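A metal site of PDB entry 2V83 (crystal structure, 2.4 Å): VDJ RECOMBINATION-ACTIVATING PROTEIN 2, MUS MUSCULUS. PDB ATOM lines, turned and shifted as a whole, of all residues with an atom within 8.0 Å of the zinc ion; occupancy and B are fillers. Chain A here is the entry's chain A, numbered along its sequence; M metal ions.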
ATOM      1  N   TYR A  10       1.028  15.874  -9.783  1.00  0.00           N
ATOM      2  CA  TYR A  10       1.789  15.072  -8.830  1.00  0.00           C
ATOM      3  C   TYR A  10       1.286  13.670  -8.570  1.00  0.00           C
ATOM      4  O   TYR A  10       2.067  12.736  -8.428  1.00  0.00           O
ATOM      5  CB  TYR A  10       1.883  15.773  -7.468  1.00  0.00           C
ATOM      6  CG  TYR A  10       2.929  16.832  -7.398  1.00  0.00           C
ATOM      7  CD1 TYR A  10       2.596  18.163  -7.564  1.00  0.00           C
ATOM      8  CD2 TYR A  10       4.259  16.507  -7.157  1.00  0.00           C
ATOM      9  CE1 TYR A  10       3.559  19.165  -7.490  1.00  0.00           C
ATOM     10  CE2 TYR A  10       5.246  17.506  -7.076  1.00  0.00           C
ATOM     11  CZ  TYR A  10       4.879  18.833  -7.243  1.00  0.00           C
ATOM     12  OH  TYR A  10       5.807  19.846  -7.175  1.00  0.00           O
ATOM     13  N   TRP A  11      -0.031  13.523  -8.502  1.00  0.00           N
ATOM     14  CA  TRP A  11      -0.626  12.227  -8.204  1.00  0.00           C
ATOM     15  C   TRP A  11      -1.092  11.439  -9.405  1.00  0.00           C
ATOM     16  O   TRP A  11      -2.172  10.835  -9.409  1.00  0.00           O
ATOM     17  CB  TRP A  11      -1.763  12.440  -7.207  1.00  0.00           C
ATOM     18  CG  TRP A  11      -1.299  13.274  -6.063  1.00  0.00           C
ATOM     19  CD1 TRP A  11      -1.674  14.553  -5.780  1.00  0.00           C
ATOM     20  CD2 TRP A  11      -0.348  12.905  -5.067  1.00  0.00           C
ATOM     21  NE1 TRP A  11      -1.003  15.014  -4.679  1.00  0.00           N
ATOM     22  CE2 TRP A  11      -0.179  14.023  -4.216  1.00  0.00           C
ATOM     23  CE3 TRP A  11       0.397  11.737  -4.812  1.00  0.00           C
ATOM     24  CZ2 TRP A  11       0.699  14.010  -3.126  1.00  0.00           C
ATOM     25  CZ3 TRP A  11       1.270  11.729  -3.729  1.00  0.00           C
ATOM     26  CH2 TRP A  11       1.404  12.860  -2.898  1.00  0.00           C
ATOM     27  N   ILE A  12      -0.262  11.453 -10.447  1.00  0.00           N
ATOM     28  CA  ILE A  12      -0.541  10.709 -11.668  1.00  0.00           C
ATOM     29  C   ILE A  12       0.143   9.355 -11.552  1.00  0.00           C
ATOM     30  O   ILE A  12       1.013   9.163 -10.692  1.00  0.00           O
ATOM     31  CB  ILE A  12       0.068  11.412 -12.886  1.00  0.00           C
ATOM     32  CG1 ILE A  12       1.590  11.472 -12.745  1.00  0.00           C
ATOM     33  CG2 ILE A  12      -0.504  12.820 -13.021  1.00  0.00           C
ATOM     34  CD1 ILE A  12       2.338  11.638 -14.049  1.00  0.00           C
ATOM     35  N   THR A  13      -0.250   8.417 -12.404  1.00  0.00           N
ATOM     36  CA  THR A  13       0.386   7.116 -12.438  1.00  0.00           C
ATOM     37  C   THR A  13       1.396   7.365 -13.554  1.00  0.00           C
ATOM     38  O   THR A  13       1.034   7.391 -14.728  1.00  0.00           O
ATOM     39  CB  THR A  13      -0.631   6.010 -12.816  1.00  0.00           C
ATOM     40  OG1 THR A  13      -1.641   5.943 -11.799  1.00  0.00           O
ATOM     41  CG2 THR A  13       0.060   4.644 -12.931  1.00  0.00           C
ATOM     42  N   CYS A  14       2.657   7.566 -13.192  1.00  0.00           N
ATOM     43  CA  CYS A  14       3.706   7.916 -14.147  1.00  0.00           C
ATOM     44  C   CYS A  14       4.248   6.838 -15.091  1.00  0.00           C
ATOM     45  O   CYS A  14       4.889   7.157 -16.092  1.00  0.00           O
ATOM     46  CB  CYS A  14       4.878   8.575 -13.403  1.00  0.00           C
ATOM     47  SG  CYS A  14       5.942   7.437 -12.495  1.00  0.00           S
ATOM     48  N   CYS A  15       4.009   5.573 -14.763  1.00  0.00           N
ATOM     49  CA  CYS A  15       4.502   4.496 -15.614  1.00  0.00           C
ATOM     50  C   CYS A  15       3.846   3.197 -15.152  1.00  0.00           C
ATOM     51  O   CYS A  15       3.397   3.093 -14.007  1.00  0.00           O
ATOM     52  CB  CYS A  15       6.025   4.408 -15.504  1.00  0.00           C
ATOM     53  SG  CYS A  15       6.591   3.878 -13.879  1.00  0.00           S
ATOM     54  N   PRO A  16       3.819   2.174 -16.022  1.00  0.00           N
ATOM     55  CA  PRO A  16       3.206   0.883 -15.688  1.00  0.00           C
ATOM     56  C   PRO A  16       3.526   0.318 -14.308  1.00  0.00           C
ATOM     57  O   PRO A  16       2.716  -0.425 -13.750  1.00  0.00           O
ATOM     58  CB  PRO A  16       3.698  -0.030 -16.806  1.00  0.00           C
ATOM     59  CG  PRO A  16       3.834   0.910 -17.969  1.00  0.00           C
ATOM     60  CD  PRO A  16       4.494   2.113 -17.329  1.00  0.00           C
ATOM     61  N   THR A  17       4.684   0.650 -13.739  1.00  0.00           N
ATOM     62  CA  THR A  17       5.054   0.125 -12.424  1.00  0.00           C
ATOM     63  C   THR A  17       4.987   1.163 -11.316  1.00  0.00           C
ATOM     64  O   THR A  17       5.467   0.914 -10.212  1.00  0.00           O
ATOM     65  CB  THR A  17       6.476  -0.448 -12.429  1.00  0.00           C
ATOM     66  OG1 THR A  17       7.372   0.516 -13.000  1.00  0.00           O
ATOM     67  CG2 THR A  17       6.545  -1.740 -13.227  1.00  0.00           C
ATOM     68  N   CYS A  18       4.377   2.304 -11.610  1.00  0.00           N
ATOM     69  CA  CYS A  18       4.274   3.402 -10.658  1.00  0.00           C
ATOM     70  C   CYS A  18       3.784   3.020  -9.257  1.00  0.00           C
ATOM     71  O   CYS A  18       2.719   2.405  -9.111  1.00  0.00           O
ATOM     72  CB  CYS A  18       3.369   4.485 -11.243  1.00  0.00           C
ATOM     73  SG  CYS A  18       3.147   5.948 -10.226  1.00  0.00           S
ATOM     74  N   ASP A  19       4.569   3.381  -8.243  1.00  0.00           N
ATOM     75  CA  ASP A  19       4.223   3.091  -6.847  1.00  0.00           C
ATOM     76  C   ASP A  19       3.789   4.309  -6.073  1.00  0.00           C
ATOM     77  O   ASP A  19       3.461   4.210  -4.896  1.00  0.00           O
ATOM     78  CB  ASP A  19       5.397   2.480  -6.110  1.00  0.00           C
ATOM     79  CG  ASP A  19       5.652   1.063  -6.474  1.00  0.00           C
ATOM     80  OD1 ASP A  19       4.664   0.323  -6.692  1.00  0.00           O
ATOM     81  OD2 ASP A  19       6.844   0.684  -6.544  1.00  0.00           O
ATOM     82  N   VAL A  20       3.795   5.471  -6.707  1.00  0.00           N
ATOM     83  CA  VAL A  20       3.376   6.670  -6.007  1.00  0.00           C
ATOM     84  C   VAL A  20       1.859   6.720  -5.980  1.00  0.00           C
ATOM     85  O   VAL A  20       1.194   6.726  -7.011  1.00  0.00           O
ATOM     86  CB  VAL A  20       3.943   7.929  -6.677  1.00  0.00           C
ATOM     87  CG1 VAL A  20       3.479   9.173  -5.948  1.00  0.00           C
ATOM     88  CG2 VAL A  20       5.460   7.872  -6.662  1.00  0.00           C
ATOM     89  N   ASP A  21       1.295   6.734  -4.780  1.00  0.00           N
ATOM     90  CA  ASP A  21      -0.144   6.772  -4.618  1.00  0.00           C
ATOM     91  C   ASP A  21      -0.517   7.799  -3.545  1.00  0.00           C
ATOM     92  O   ASP A  21       0.057   7.825  -2.452  1.00  0.00           O
ATOM     93  CB  ASP A  21      -0.651   5.378  -4.257  1.00  0.00           C
ATOM     94  CG  ASP A  21      -2.147   5.328  -4.059  1.00  0.00           C
ATOM     95  OD1 ASP A  21      -2.862   6.113  -4.727  1.00  0.00           O
ATOM     96  OD2 ASP A  21      -2.625   4.499  -3.254  1.00  0.00           O
ATOM     97  N   PRO A  36       5.994  14.309  -3.806  1.00  0.00           N
ATOM     98  CA  PRO A  36       6.975  13.439  -4.468  1.00  0.00           C
ATOM     99  C   PRO A  36       7.834  14.150  -5.496  1.00  0.00           C
ATOM    100  O   PRO A  36       7.333  14.916  -6.315  1.00  0.00           O
ATOM    101  CB  PRO A  36       6.101  12.359  -5.084  1.00  0.00           C
ATOM    102  CG  PRO A  36       4.865  13.125  -5.481  1.00  0.00           C
ATOM    103  CD  PRO A  36       4.627  14.026  -4.283  1.00  0.00           C
ATOM    104  N   ALA A  37       9.130  13.878  -5.447  1.00  0.00           N
ATOM    105  CA  ALA A  37      10.071  14.478  -6.384  1.00  0.00           C
ATOM    106  C   ALA A  37       9.768  13.939  -7.758  1.00  0.00           C
ATOM    107  O   ALA A  37       9.483  12.749  -7.920  1.00  0.00           O
ATOM    108  CB  ALA A  37      11.498  14.138  -5.980  1.00  0.00           C
ATOM    109  N   MET A  38       9.842  14.806  -8.762  1.00  0.00           N
ATOM    110  CA  MET A  38       9.576  14.373 -10.126  1.00  0.00           C
ATOM    111  C   MET A  38      10.661  14.855 -11.081  1.00  0.00           C
ATOM    112  O   MET A  38      11.360  15.841 -10.819  1.00  0.00           O
ATOM    113  CB  MET A  38       8.199  14.890 -10.573  1.00  0.00           C
ATOM    114  CG  MET A  38       7.062  14.371  -9.703  1.00  0.00           C
ATOM    115  SD  MET A  38       5.419  14.789 -10.298  1.00  0.00           S
ATOM    116  CE  MET A  38       5.056  13.381 -11.255  1.00  0.00           C
ATOM    117  N   TRP A  48       6.116  13.857 -17.278  1.00  0.00           N
ATOM    118  CA  TRP A  48       6.702  13.801 -15.948  1.00  0.00           C
ATOM    119  C   TRP A  48       6.586  12.429 -15.284  1.00  0.00           C
ATOM    120  O   TRP A  48       5.549  11.758 -15.391  1.00  0.00           O
ATOM    121  CB  TRP A  48       6.037  14.825 -15.021  1.00  0.00           C
ATOM    122  CG  TRP A  48       6.309  16.246 -15.345  1.00  0.00           C
ATOM    123  CD1 TRP A  48       5.597  17.048 -16.189  1.00  0.00           C
ATOM    124  CD2 TRP A  48       7.376  17.066 -14.834  1.00  0.00           C
ATOM    125  NE1 TRP A  48       6.154  18.313 -16.242  1.00  0.00           N
ATOM    126  CE2 TRP A  48       7.243  18.347 -15.407  1.00  0.00           C
ATOM    127  CE3 TRP A  48       8.428  16.829 -13.929  1.00  0.00           C
ATOM    128  CZ2 TRP A  48       8.123  19.386 -15.120  1.00  0.00           C
ATOM    129  CZ3 TRP A  48       9.302  17.872 -13.649  1.00  0.00           C
ATOM    130  CH2 TRP A  48       9.142  19.137 -14.239  1.00  0.00           C
ATOM    131  N   VAL A  49       7.629  12.010 -14.596  1.00  0.00           N
ATOM    132  CA  VAL A  49       7.606  10.748 -13.864  1.00  0.00           C
ATOM    133  C   VAL A  49       8.109  10.971 -12.439  1.00  0.00           C
ATOM    134  O   VAL A  49       8.797  11.949 -12.157  1.00  0.00           O
ATOM    135  CB  VAL A  49       8.494   9.690 -14.542  1.00  0.00           C
ATOM    136  CG1 VAL A  49       7.893   9.300 -15.888  1.00  0.00           C
ATOM    137  CG2 VAL A  49       9.926  10.219 -14.705  1.00  0.00           C
ATOM    138  N   HIS A  50       7.720  10.084 -11.527  1.00  0.00           N
ATOM    139  CA  HIS A  50       8.185  10.209 -10.155  1.00  0.00           C
ATOM    140  C   HIS A  50       9.588   9.641 -10.124  1.00  0.00           C
ATOM    141  O   HIS A  50       9.820   8.528 -10.604  1.00  0.00           O
ATOM    142  CB  HIS A  50       7.289   9.415  -9.198  1.00  0.00           C
ATOM    143  CG  HIS A  50       5.842   9.820  -9.227  1.00  0.00           C
ATOM    144  ND1 HIS A  50       4.845   8.986  -9.689  1.00  0.00           N
ATOM    145  CD2 HIS A  50       5.221  10.951  -8.806  1.00  0.00           C
ATOM    146  CE1 HIS A  50       3.673   9.588  -9.554  1.00  0.00           C
ATOM    147  NE2 HIS A  50       3.879  10.772  -9.014  1.00  0.00           N
ATOM    148  N   ALA A  51      10.537  10.396  -9.582  1.00  0.00           N
ATOM    149  CA  ALA A  51      11.923   9.949  -9.511  1.00  0.00           C
ATOM    150  C   ALA A  51      12.084   8.588  -8.835  1.00  0.00           C
ATOM    151  O   ALA A  51      12.866   7.753  -9.285  1.00  0.00           O
ATOM    152  CB  ALA A  51      12.762  10.996  -8.779  1.00  0.00           C
ATOM    153  N   GLN A  52      11.322   8.364  -7.763  1.00  0.00           N
ATOM    154  CA  GLN A  52      11.415   7.103  -7.029  1.00  0.00           C
ATOM    155  C   GLN A  52      11.007   5.930  -7.898  1.00  0.00           C
ATOM    156  O   GLN A  52      11.565   4.839  -7.784  1.00  0.00           O
ATOM    157  CB  GLN A  52      10.516   7.154  -5.784  1.00  0.00           C
ATOM    158  CG  GLN A  52      10.937   6.170  -4.707  1.00  0.00           C
ATOM    159  CD  GLN A  52      10.052   6.203  -3.472  1.00  0.00           C
ATOM    160  OE1 GLN A  52       9.360   7.192  -3.211  1.00  0.00           O
ATOM    161  NE2 GLN A  52      10.076   5.128  -2.695  1.00  0.00           N
ATOM    162  N   CYS A  53      10.037   6.148  -8.769  1.00  0.00           N
ATOM    163  CA  CYS A  53       9.568   5.085  -9.657  1.00  0.00           C
ATOM    164  C   CYS A  53      10.627   4.712 -10.681  1.00  0.00           C
ATOM    165  O   CYS A  53      10.556   3.661 -11.298  1.00  0.00           O
ATOM    166  CB  CYS A  53       8.293   5.503 -10.363  1.00  0.00           C
ATOM    167  SG  CYS A  53       6.934   5.824  -9.237  1.00  0.00           S
ATOM    168  N   MET A  54      11.614   5.580 -10.865  1.00  0.00           N
ATOM    169  CA  MET A  54      12.686   5.307 -11.829  1.00  0.00           C
ATOM    170  C   MET A  54      13.865   4.653 -11.127  1.00  0.00           C
ATOM    171  O   MET A  54      14.856   4.291 -11.770  1.00  0.00           O
ATOM    172  CB  MET A  54      13.145   6.605 -12.493  1.00  0.00           C
ATOM    173  CG  MET A  54      12.052   7.354 -13.222  1.00  0.00           C
ATOM    174  SD  MET A  54      11.414   6.459 -14.650  1.00  0.00           S
ATOM    175  CE  MET A  54       9.806   5.906 -14.078  1.00  0.00           C
HETATM  176 ZN    ZN M   1       5.300   7.049 -10.323  1.00  0.00          ZN
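The backbone NH of Cys 18 lies within hydrogen-bond range of the side-chain sulfur of Cys 15 (3.5 Å).
N of Asp 19 lies close to SG of Cys 53 (3.5 Å).
N of Val 20 sits close to SG of Cys 18, 3.6 Å away.
A ring nitrogen (NE2) of His 50 is in hydrogen-bond range of the backbone carbonyl oxygen (O) of Tyr 10 (2.7 Å).
The zinc ion is bound by ND1 of His 50 (2.1 Å), SG of Cys 14 (2.3 Å), SG of Cys 53 (2.3 Å) and SG of Cys 18 (2.4 Å).
Val 20 touches the zinc ion (CG2 to ZN, 3.8 Å).
The nearest printed residue that does not touch the zinc ion is Asp 19 (4.3 Å).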
